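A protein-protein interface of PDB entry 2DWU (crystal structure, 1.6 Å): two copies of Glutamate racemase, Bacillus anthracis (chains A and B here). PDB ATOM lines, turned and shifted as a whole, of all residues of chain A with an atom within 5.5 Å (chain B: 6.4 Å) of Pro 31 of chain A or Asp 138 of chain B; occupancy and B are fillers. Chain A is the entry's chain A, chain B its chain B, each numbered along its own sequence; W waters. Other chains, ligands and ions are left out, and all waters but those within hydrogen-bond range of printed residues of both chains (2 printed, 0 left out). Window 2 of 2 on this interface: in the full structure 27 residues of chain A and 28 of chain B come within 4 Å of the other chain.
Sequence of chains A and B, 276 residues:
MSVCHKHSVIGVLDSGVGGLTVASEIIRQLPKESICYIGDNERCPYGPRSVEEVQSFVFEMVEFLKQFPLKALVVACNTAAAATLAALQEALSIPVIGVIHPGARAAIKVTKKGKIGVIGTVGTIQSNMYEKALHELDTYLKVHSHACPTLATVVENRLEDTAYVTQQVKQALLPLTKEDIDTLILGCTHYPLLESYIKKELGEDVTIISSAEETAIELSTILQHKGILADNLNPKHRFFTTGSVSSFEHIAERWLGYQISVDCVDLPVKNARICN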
ATOM      1  N   ILE A  26      21.718  18.166  -1.289  1.00  0.00           N
ATOM      2  CA  ILE A  26      21.791  16.753  -1.672  1.00  0.00           C
ATOM      3  C   ILE A  26      20.390  16.136  -1.560  1.00  0.00           C
ATOM      4  O   ILE A  26      19.933  15.423  -2.453  1.00  0.00           O
ATOM      5  CB  ILE A  26      22.787  15.987  -0.793  1.00  0.00           C
ATOM      6  CG1 ILE A  26      24.208  16.524  -1.067  1.00  0.00           C
ATOM      7  CG2 ILE A  26      22.685  14.480  -1.064  1.00  0.00           C
ATOM      8  CD1 ILE A  26      25.269  15.977  -0.086  1.00  0.00           C
ATOM      9  N   ILE A  27      19.686  16.460  -0.478  1.00  0.00           N
ATOM     10  CA  ILE A  27      18.324  15.952  -0.307  1.00  0.00           C
ATOM     11  C   ILE A  27      17.415  16.437  -1.447  1.00  0.00           C
ATOM     12  O   ILE A  27      16.563  15.690  -1.953  1.00  0.00           O
ATOM     13  CB  ILE A  27      17.773  16.407   1.080  1.00  0.00           C
ATOM     14  CG1 ILE A  27      18.520  15.638   2.172  1.00  0.00           C
ATOM     15  CG2 ILE A  27      16.229  16.244   1.133  1.00  0.00           C
ATOM     16  CD1 ILE A  27      18.301  16.213   3.573  1.00  0.00           C
ATOM     17  N   ARG A  28      17.614  17.670  -1.904  1.00  0.00           N
ATOM     18  CA  ARG A  28      16.773  18.198  -2.964  1.00  0.00           C
ATOM     19  C   ARG A  28      17.092  17.648  -4.360  1.00  0.00           C
ATOM     20  O   ARG A  28      16.185  17.288  -5.115  1.00  0.00           O
ATOM     21  CB  ARG A  28      16.882  19.729  -2.988  1.00  0.00           C
ATOM     22  CG  ARG A  28      15.918  20.454  -3.970  1.00  0.00           C
ATOM     23  CD  ARG A  28      16.084  21.984  -3.884  1.00  0.00           C
ATOM     24  NE  ARG A  28      17.336  22.455  -4.464  1.00  0.00           N
ATOM     25  CZ  ARG A  28      17.561  22.539  -5.766  1.00  0.00           C
ATOM     26  NH1 ARG A  28      16.602  22.192  -6.631  1.00  0.00           N
ATOM     27  NH2 ARG A  28      18.752  22.944  -6.190  1.00  0.00           N
ATOM     28  N   GLN A  29      18.374  17.605  -4.720  1.00  0.00           N
ATOM     29  CA  GLN A  29      18.772  17.167  -6.059  1.00  0.00           C
ATOM     30  C   GLN A  29      18.967  15.656  -6.206  1.00  0.00           C
ATOM     31  O   GLN A  29      18.955  15.125  -7.317  1.00  0.00           O
ATOM     32  CB  GLN A  29      20.063  17.892  -6.460  1.00  0.00           C
ATOM     33  CG  GLN A  29      19.916  19.394  -6.520  1.00  0.00           C
ATOM     34  CD  GLN A  29      21.182  20.041  -7.051  1.00  0.00           C
ATOM     35  OE1 GLN A  29      21.682  19.627  -8.086  1.00  0.00           O
ATOM     36  NE2 GLN A  29      21.719  21.030  -6.330  1.00  0.00           N
ATOM     37  N   LEU A  30      19.119  14.963  -5.087  1.00  0.00           N
ATOM     38  CA  LEU A  30      19.290  13.500  -5.114  1.00  0.00           C
ATOM     39  C   LEU A  30      18.322  12.954  -4.066  1.00  0.00           C
ATOM     40  O   LEU A  30      18.731  12.329  -3.083  1.00  0.00           O
ATOM     41  CB  LEU A  30      20.728  13.143  -4.750  1.00  0.00           C
ATOM     42  CG  LEU A  30      21.749  13.327  -5.890  1.00  0.00           C
ATOM     43  CD1 LEU A  30      23.185  13.300  -5.347  1.00  0.00           C
ATOM     44  CD2 LEU A  30      21.525  12.232  -6.915  1.00  0.00           C
ATOM     45  N   PRO A  31      17.025  13.148  -4.310  1.00  0.00           N
ATOM     46  CA  PRO A  31      16.001  12.699  -3.360  1.00  0.00           C
ATOM     47  C   PRO A  31      15.893  11.229  -3.081  1.00  0.00           C
ATOM     48  O   PRO A  31      15.160  10.847  -2.162  1.00  0.00           O
ATOM     49  CB  PRO A  31      14.714  13.299  -3.922  1.00  0.00           C
ATOM     50  CG  PRO A  31      14.956  13.295  -5.419  1.00  0.00           C
ATOM     51  CD  PRO A  31      16.424  13.736  -5.520  1.00  0.00           C
ATOM     52  N   LYS A  32      16.600  10.388  -3.826  1.00  0.00           N
ATOM     53  CA  LYS A  32      16.548   8.947  -3.528  1.00  0.00           C
ATOM     54  C   LYS A  32      17.707   8.480  -2.652  1.00  0.00           C
ATOM     55  O   LYS A  32      17.719   7.341  -2.188  1.00  0.00           O
ATOM     56  CB  LYS A  32      16.518   8.118  -4.811  1.00  0.00           C
ATOM     57  CG  LYS A  32      15.342   8.473  -5.710  1.00  0.00           C
ATOM     58  CD  LYS A  32      15.342   7.634  -6.950  1.00  0.00           C
ATOM     59  CE  LYS A  32      14.230   8.090  -7.882  1.00  0.00           C
ATOM     60  NZ  LYS A  32      14.127   7.217  -9.092  1.00  0.00           N
ATOM     61  N   GLU A  33      18.683   9.354  -2.413  1.00  0.00           N
ATOM     62  CA  GLU A  33      19.846   8.998  -1.598  1.00  0.00           C
ATOM     63  C   GLU A  33      19.575   9.216  -0.104  1.00  0.00           C
ATOM     64  O   GLU A  33      18.731  10.039   0.268  1.00  0.00           O
ATOM     65  CB  GLU A  33      21.048   9.848  -2.014  1.00  0.00           C
ATOM     66  CG  GLU A  33      21.437   9.698  -3.486  1.00  0.00           C
ATOM     67  CD  GLU A  33      21.962   8.319  -3.866  1.00  0.00           C
ATOM     68  OE1 GLU A  33      22.505   7.588  -3.000  1.00  0.00           O
ATOM     69  OE2 GLU A  33      21.858   7.958  -5.068  1.00  0.00           O
ATOM     70  N   ASN A 232      15.716   4.372  -4.039  1.00  0.00           N
ATOM     71  CA  ASN A 232      14.798   4.514  -2.892  1.00  0.00           C
ATOM     72  C   ASN A 232      13.800   5.683  -3.032  1.00  0.00           C
ATOM     73  O   ASN A 232      14.199   6.845  -3.058  1.00  0.00           O
ATOM     74  CB  ASN A 232      15.666   4.732  -1.655  1.00  0.00           C
ATOM     75  CG  ASN A 232      14.917   4.537  -0.362  1.00  0.00           C
ATOM     76  OD1 ASN A 232      13.693   4.675  -0.298  1.00  0.00           O
ATOM     77  ND2 ASN A 232      15.670   4.243   0.699  1.00  0.00           N
ATOM     78  N   LEU A 233      12.504   5.369  -3.072  1.00  0.00           N
ATOM     79  CA  LEU A 233      11.474   6.399  -3.231  1.00  0.00           C
ATOM     80  C   LEU A 233      11.129   7.205  -1.979  1.00  0.00           C
ATOM     81  O   LEU A 233      10.414   8.216  -2.067  1.00  0.00           O
ATOM     82  CB  LEU A 233      10.195   5.779  -3.811  1.00  0.00           C
ATOM     83  CG  LEU A 233      10.352   5.071  -5.160  1.00  0.00           C
ATOM     84  CD1 LEU A 233       9.013   4.484  -5.574  1.00  0.00           C
ATOM     85  CD2 LEU A 233      10.851   6.044  -6.227  1.00  0.00           C
ATOM     86  N   PRO A 235      13.669   7.752   1.276  1.00  0.00           N
ATOM     87  CA  PRO A 235      14.747   7.509   2.231  1.00  0.00           C
ATOM     88  C   PRO A 235      14.576   8.341   3.493  1.00  0.00           C
ATOM     89  O   PRO A 235      13.744   9.243   3.551  1.00  0.00           O
ATOM     90  CB  PRO A 235      15.995   7.915   1.450  1.00  0.00           C
ATOM     91  CG  PRO A 235      15.488   9.056   0.596  1.00  0.00           C
ATOM     92  CD  PRO A 235      14.135   8.534   0.114  1.00  0.00           C
ATOM     93  N   ILE B 108      17.114  19.497 -12.773  1.00  0.00           N
ATOM     94  CA  ILE B 108      16.777  19.167 -11.381  1.00  0.00           C
ATOM     95  C   ILE B 108      17.382  20.224 -10.451  1.00  0.00           C
ATOM     96  O   ILE B 108      16.778  20.619  -9.450  1.00  0.00           O
ATOM     97  CB  ILE B 108      17.298  17.741 -11.026  1.00  0.00           C
ATOM     98  CG1 ILE B 108      16.396  16.713 -11.734  1.00  0.00           C
ATOM     99  CG2 ILE B 108      17.271  17.483  -9.518  1.00  0.00           C
ATOM    100  CD1 ILE B 108      16.839  15.276 -11.572  1.00  0.00           C
ATOM    101  N   GLY B 114       9.520  21.435  -9.709  1.00  0.00           N
ATOM    102  CA  GLY B 114       9.631  20.064 -10.154  1.00  0.00           C
ATOM    103  C   GLY B 114       8.822  19.808 -11.415  1.00  0.00           C
ATOM    104  O   GLY B 114       8.353  18.712 -11.607  1.00  0.00           O
ATOM    105  N   ALA B 133      15.564   9.737 -17.866  1.00  0.00           N
ATOM    106  CA  ALA B 133      16.719  10.217 -17.117  1.00  0.00           C
ATOM    107  C   ALA B 133      16.302  11.035 -15.907  1.00  0.00           C
ATOM    108  O   ALA B 133      16.899  10.917 -14.824  1.00  0.00           O
ATOM    109  CB  ALA B 133      17.627  11.062 -18.026  1.00  0.00           C
ATOM    110  N   LEU B 134      15.313  11.895 -16.104  1.00  0.00           N
ATOM    111  CA  LEU B 134      14.838  12.721 -15.020  1.00  0.00           C
ATOM    112  C   LEU B 134      14.259  11.872 -13.896  1.00  0.00           C
ATOM    113  O   LEU B 134      14.575  12.104 -12.724  1.00  0.00           O
ATOM    114  CB  LEU B 134      13.796  13.720 -15.525  1.00  0.00           C
ATOM    115  CG  LEU B 134      14.426  14.905 -16.296  1.00  0.00           C
ATOM    116  CD1 LEU B 134      13.369  15.636 -17.144  1.00  0.00           C
ATOM    117  CD2 LEU B 134      15.061  15.839 -15.263  1.00  0.00           C
ATOM    118  N   HIS B 135      13.445  10.885 -14.253  1.00  0.00           N
ATOM    119  CA  HIS B 135      12.822  10.046 -13.226  1.00  0.00           C
ATOM    120  C   HIS B 135      13.774   9.131 -12.511  1.00  0.00           C
ATOM    121  O   HIS B 135      13.516   8.750 -11.369  1.00  0.00           O
ATOM    122  CB  HIS B 135      11.650   9.268 -13.830  1.00  0.00           C
ATOM    123  CG  HIS B 135      10.439  10.117 -14.019  1.00  0.00           C
ATOM    124  ND1 HIS B 135       9.430   9.790 -14.898  1.00  0.00           N
ATOM    125  CD2 HIS B 135      10.086  11.297 -13.461  1.00  0.00           C
ATOM    126  CE1 HIS B 135       8.508  10.739 -14.877  1.00  0.00           C
ATOM    127  NE2 HIS B 135       8.880  11.664 -14.014  1.00  0.00           N
ATOM    128  N   GLU B 136      14.888   8.821 -13.158  1.00  0.00           N
ATOM    129  CA  GLU B 136      15.900   7.993 -12.510  1.00  0.00           C
ATOM    130  C   GLU B 136      16.452   8.764 -11.318  1.00  0.00           C
ATOM    131  O   GLU B 136      16.776   8.174 -10.296  1.00  0.00           O
ATOM    132  CB  GLU B 136      17.027   7.670 -13.478  1.00  0.00           C
ATOM    133  CG  GLU B 136      18.030   6.668 -12.923  1.00  0.00           C
ATOM    134  CD  GLU B 136      19.045   6.208 -13.961  1.00  0.00           C
ATOM    135  OE1 GLU B 136      19.824   5.274 -13.659  1.00  0.00           O
ATOM    136  OE2 GLU B 136      19.074   6.770 -15.075  1.00  0.00           O
ATOM    137  N   LEU B 137      16.577  10.085 -11.445  1.00  0.00           N
ATOM    138  CA  LEU B 137      17.096  10.875 -10.338  1.00  0.00           C
ATOM    139  C   LEU B 137      15.990  11.281  -9.358  1.00  0.00           C
ATOM    140  O   LEU B 137      16.231  11.395  -8.160  1.00  0.00           O
ATOM    141  CB  LEU B 137      17.797  12.130 -10.879  1.00  0.00           C
ATOM    142  CG  LEU B 137      19.081  11.811 -11.670  1.00  0.00           C
ATOM    143  CD1 LEU B 137      19.484  13.043 -12.462  1.00  0.00           C
ATOM    144  CD2 LEU B 137      20.197  11.399 -10.730  1.00  0.00           C
ATOM    145  N   ASP B 138      14.794  11.543  -9.868  1.00  0.00           N
ATOM    146  CA  ASP B 138      13.691  11.971  -8.998  1.00  0.00           C
ATOM    147  C   ASP B 138      12.389  11.540  -9.650  1.00  0.00           C
ATOM    148  O   ASP B 138      11.949  12.111 -10.644  1.00  0.00           O
ATOM    149  CB  ASP B 138      13.687  13.504  -8.852  1.00  0.00           C
ATOM    150  CG  ASP B 138      12.633  14.016  -7.835  1.00  0.00           C
ATOM    151  OD1 ASP B 138      12.597  15.248  -7.594  1.00  0.00           O
ATOM    152  OD2 ASP B 138      11.846  13.197  -7.276  1.00  0.00           O
ATOM    153  N   THR B 139      11.787  10.516  -9.069  1.00  0.00           N
ATOM    154  CA  THR B 139      10.542   9.978  -9.589  1.00  0.00           C
ATOM    155  C   THR B 139       9.386  10.983  -9.562  1.00  0.00           C
ATOM    156  O   THR B 139       8.478  10.897 -10.404  1.00  0.00           O
ATOM    157  CB  THR B 139      10.189   8.722  -8.764  1.00  0.00           C
ATOM    158  OG1 THR B 139      11.128   7.692  -9.064  1.00  0.00           O
ATOM    159  CG2 THR B 139       8.770   8.219  -9.079  1.00  0.00           C
ATOM    160  N   TYR B 140       9.418  11.921  -8.616  1.00  0.00           N
ATOM    161  CA  TYR B 140       8.338  12.900  -8.453  1.00  0.00           C
ATOM    162  C   TYR B 140       8.489  14.219  -9.198  1.00  0.00           C
ATOM    163  O   TYR B 140       8.311  15.319  -8.638  1.00  0.00           O
ATOM    164  CB  TYR B 140       8.123  13.160  -6.960  1.00  0.00           C
ATOM    165  CG  TYR B 140       8.024  11.875  -6.165  1.00  0.00           C
ATOM    166  CD1 TYR B 140       9.049  11.496  -5.295  1.00  0.00           C
ATOM    167  CD2 TYR B 140       6.920  11.028  -6.302  1.00  0.00           C
ATOM    168  CE1 TYR B 140       8.979  10.296  -4.573  1.00  0.00           C
ATOM    169  CE2 TYR B 140       6.839   9.829  -5.586  1.00  0.00           C
ATOM    170  CZ  TYR B 140       7.875   9.474  -4.724  1.00  0.00           C
ATOM    171  OH  TYR B 140       7.809   8.303  -4.002  1.00  0.00           O
ATOM    172  N   LEU B 141       8.862  14.108 -10.463  1.00  0.00           N
ATOM    173  CA  LEU B 141       8.981  15.283 -11.317  1.00  0.00           C
ATOM    174  C   LEU B 141       7.942  15.113 -12.405  1.00  0.00           C
ATOM    175  O   LEU B 141       7.606  13.988 -12.777  1.00  0.00           O
ATOM    176  CB  LEU B 141      10.364  15.325 -11.974  1.00  0.00           C
ATOM    177  CG  LEU B 141      11.569  15.585 -11.074  1.00  0.00           C
ATOM    178  CD1 LEU B 141      12.851  15.278 -11.869  1.00  0.00           C
ATOM    179  CD2 LEU B 141      11.560  17.045 -10.576  1.00  0.00           C
HETATM  180  O   HOH W   1      14.766  16.918  -7.510  1.00  0.00           O
HETATM  181  O   HOH W   2      18.161  10.746  -6.246  1.00  0.00           O
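Water W1 lies within hydrogen-bond range of the side-chain carboxylate of Asp 138 of chain B (2.7 Å) and the backbone carbonyl oxygen of Arg 28 of chain A (2.8 Å).
Water W2 lies within hydrogen-bond range of O of Leu 137 of chain B (2.8 Å) and N of Lys 32 of chain A (2.9 Å).
The backbone carbonyl oxygen (O) of Ile 108 of chain B is in hydrogen-bond range of the guanidinium group (NH1) of Arg 28 of chain A.
The backbone carbonyl oxygen of His 135 of chain B sits at hydrogen-bond distance from the side-chain amino group of Lys 32 of chain A (2.8 Å).
The backbone carbonyl oxygen (O) of Glu 136 of chain B sits at hydrogen-bond distance from the side-chain amino group (NZ) of Lys 32 of chain A (3.1 Å).
OG1 of Thr 139 of chain B sits at hydrogen-bond distance from NZ of Lys 32 of chain A.
The backbone carbonyl oxygen of Leu 233 of chain A lies within hydrogen-bond range of the side-chain hydroxyl of Tyr 140 of chain B (3.2 Å).
Among the printed residues, merely in contact across the chains: Gln 29 of chain A with Ile 108 of chain B (3.6 Å), Pro 31 of chain A with Leu 137 of chain B (3.5 Å), Pro 31 of chain A with Asp 138 of chain B (3.4 Å), Lys 32 of chain A with Leu 137 of chain B (3.9 Å) and Leu 233 of chain A with Thr 139 of chain B (3.3 Å).
OG1 of Thr 139 of chain B is in hydrogen-bond range of O of His 135 of chain B, 3.5 Å away.
A ring nitrogen (NE2) of His 135 of chain B is in hydrogen-bond range of the backbone carbonyl oxygen of Leu 141 of chain B, at 2.9 Å.
The side-chain carboxylate (OD2) of Asp 138 of chain B is in hydrogen-bond range of the backbone NH (N) of Tyr 140 of chain B, at 3.1 Å.
Of chain B, only Leu 137 (3.5 Å) and Asp 138 (3.4 Å) come within 4 Å of Pro 31 of chain A.
Printed residues of chain A within 4 Å of Ile 108 of chain B: Arg 28 (3.2 Å) and Gln 29 (3.6 Å).
Printed residues of chain A within 4 Å of Thr 139 of chain B: Lys 32 and Leu 233.
Of the printed residues of chain B, Leu 233 of chain A touches Thr 139 (3.3 Å) and Tyr 140 (3.2 Å).
Of the printed residues of chain A, Leu 137 of chain B touches Pro 31 and Lys 32.
Printed residues of chain B within 4 Å of Lys 32 of chain A: His 135, Glu 136, Leu 137 and Thr 139.
Ile 27 of chain A touches none of the printed residues of chain B.
Leu 141 of chain B touches none of the printed residues of chain A.
The nearest residue of chain A that does not touch Asp 138 of chain B is Lys 32 of chain A (4.02 Å).
The nearest printed residue of chain B that does not touch Arg 28 of chain A is Asp 138 of chain B (4.8 Å).
No position is printed for both chains.
Hydrophobic or aromatic side chains of chain B within 4 Å of the printed part of chain A: Ile 108 and Tyr 140.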
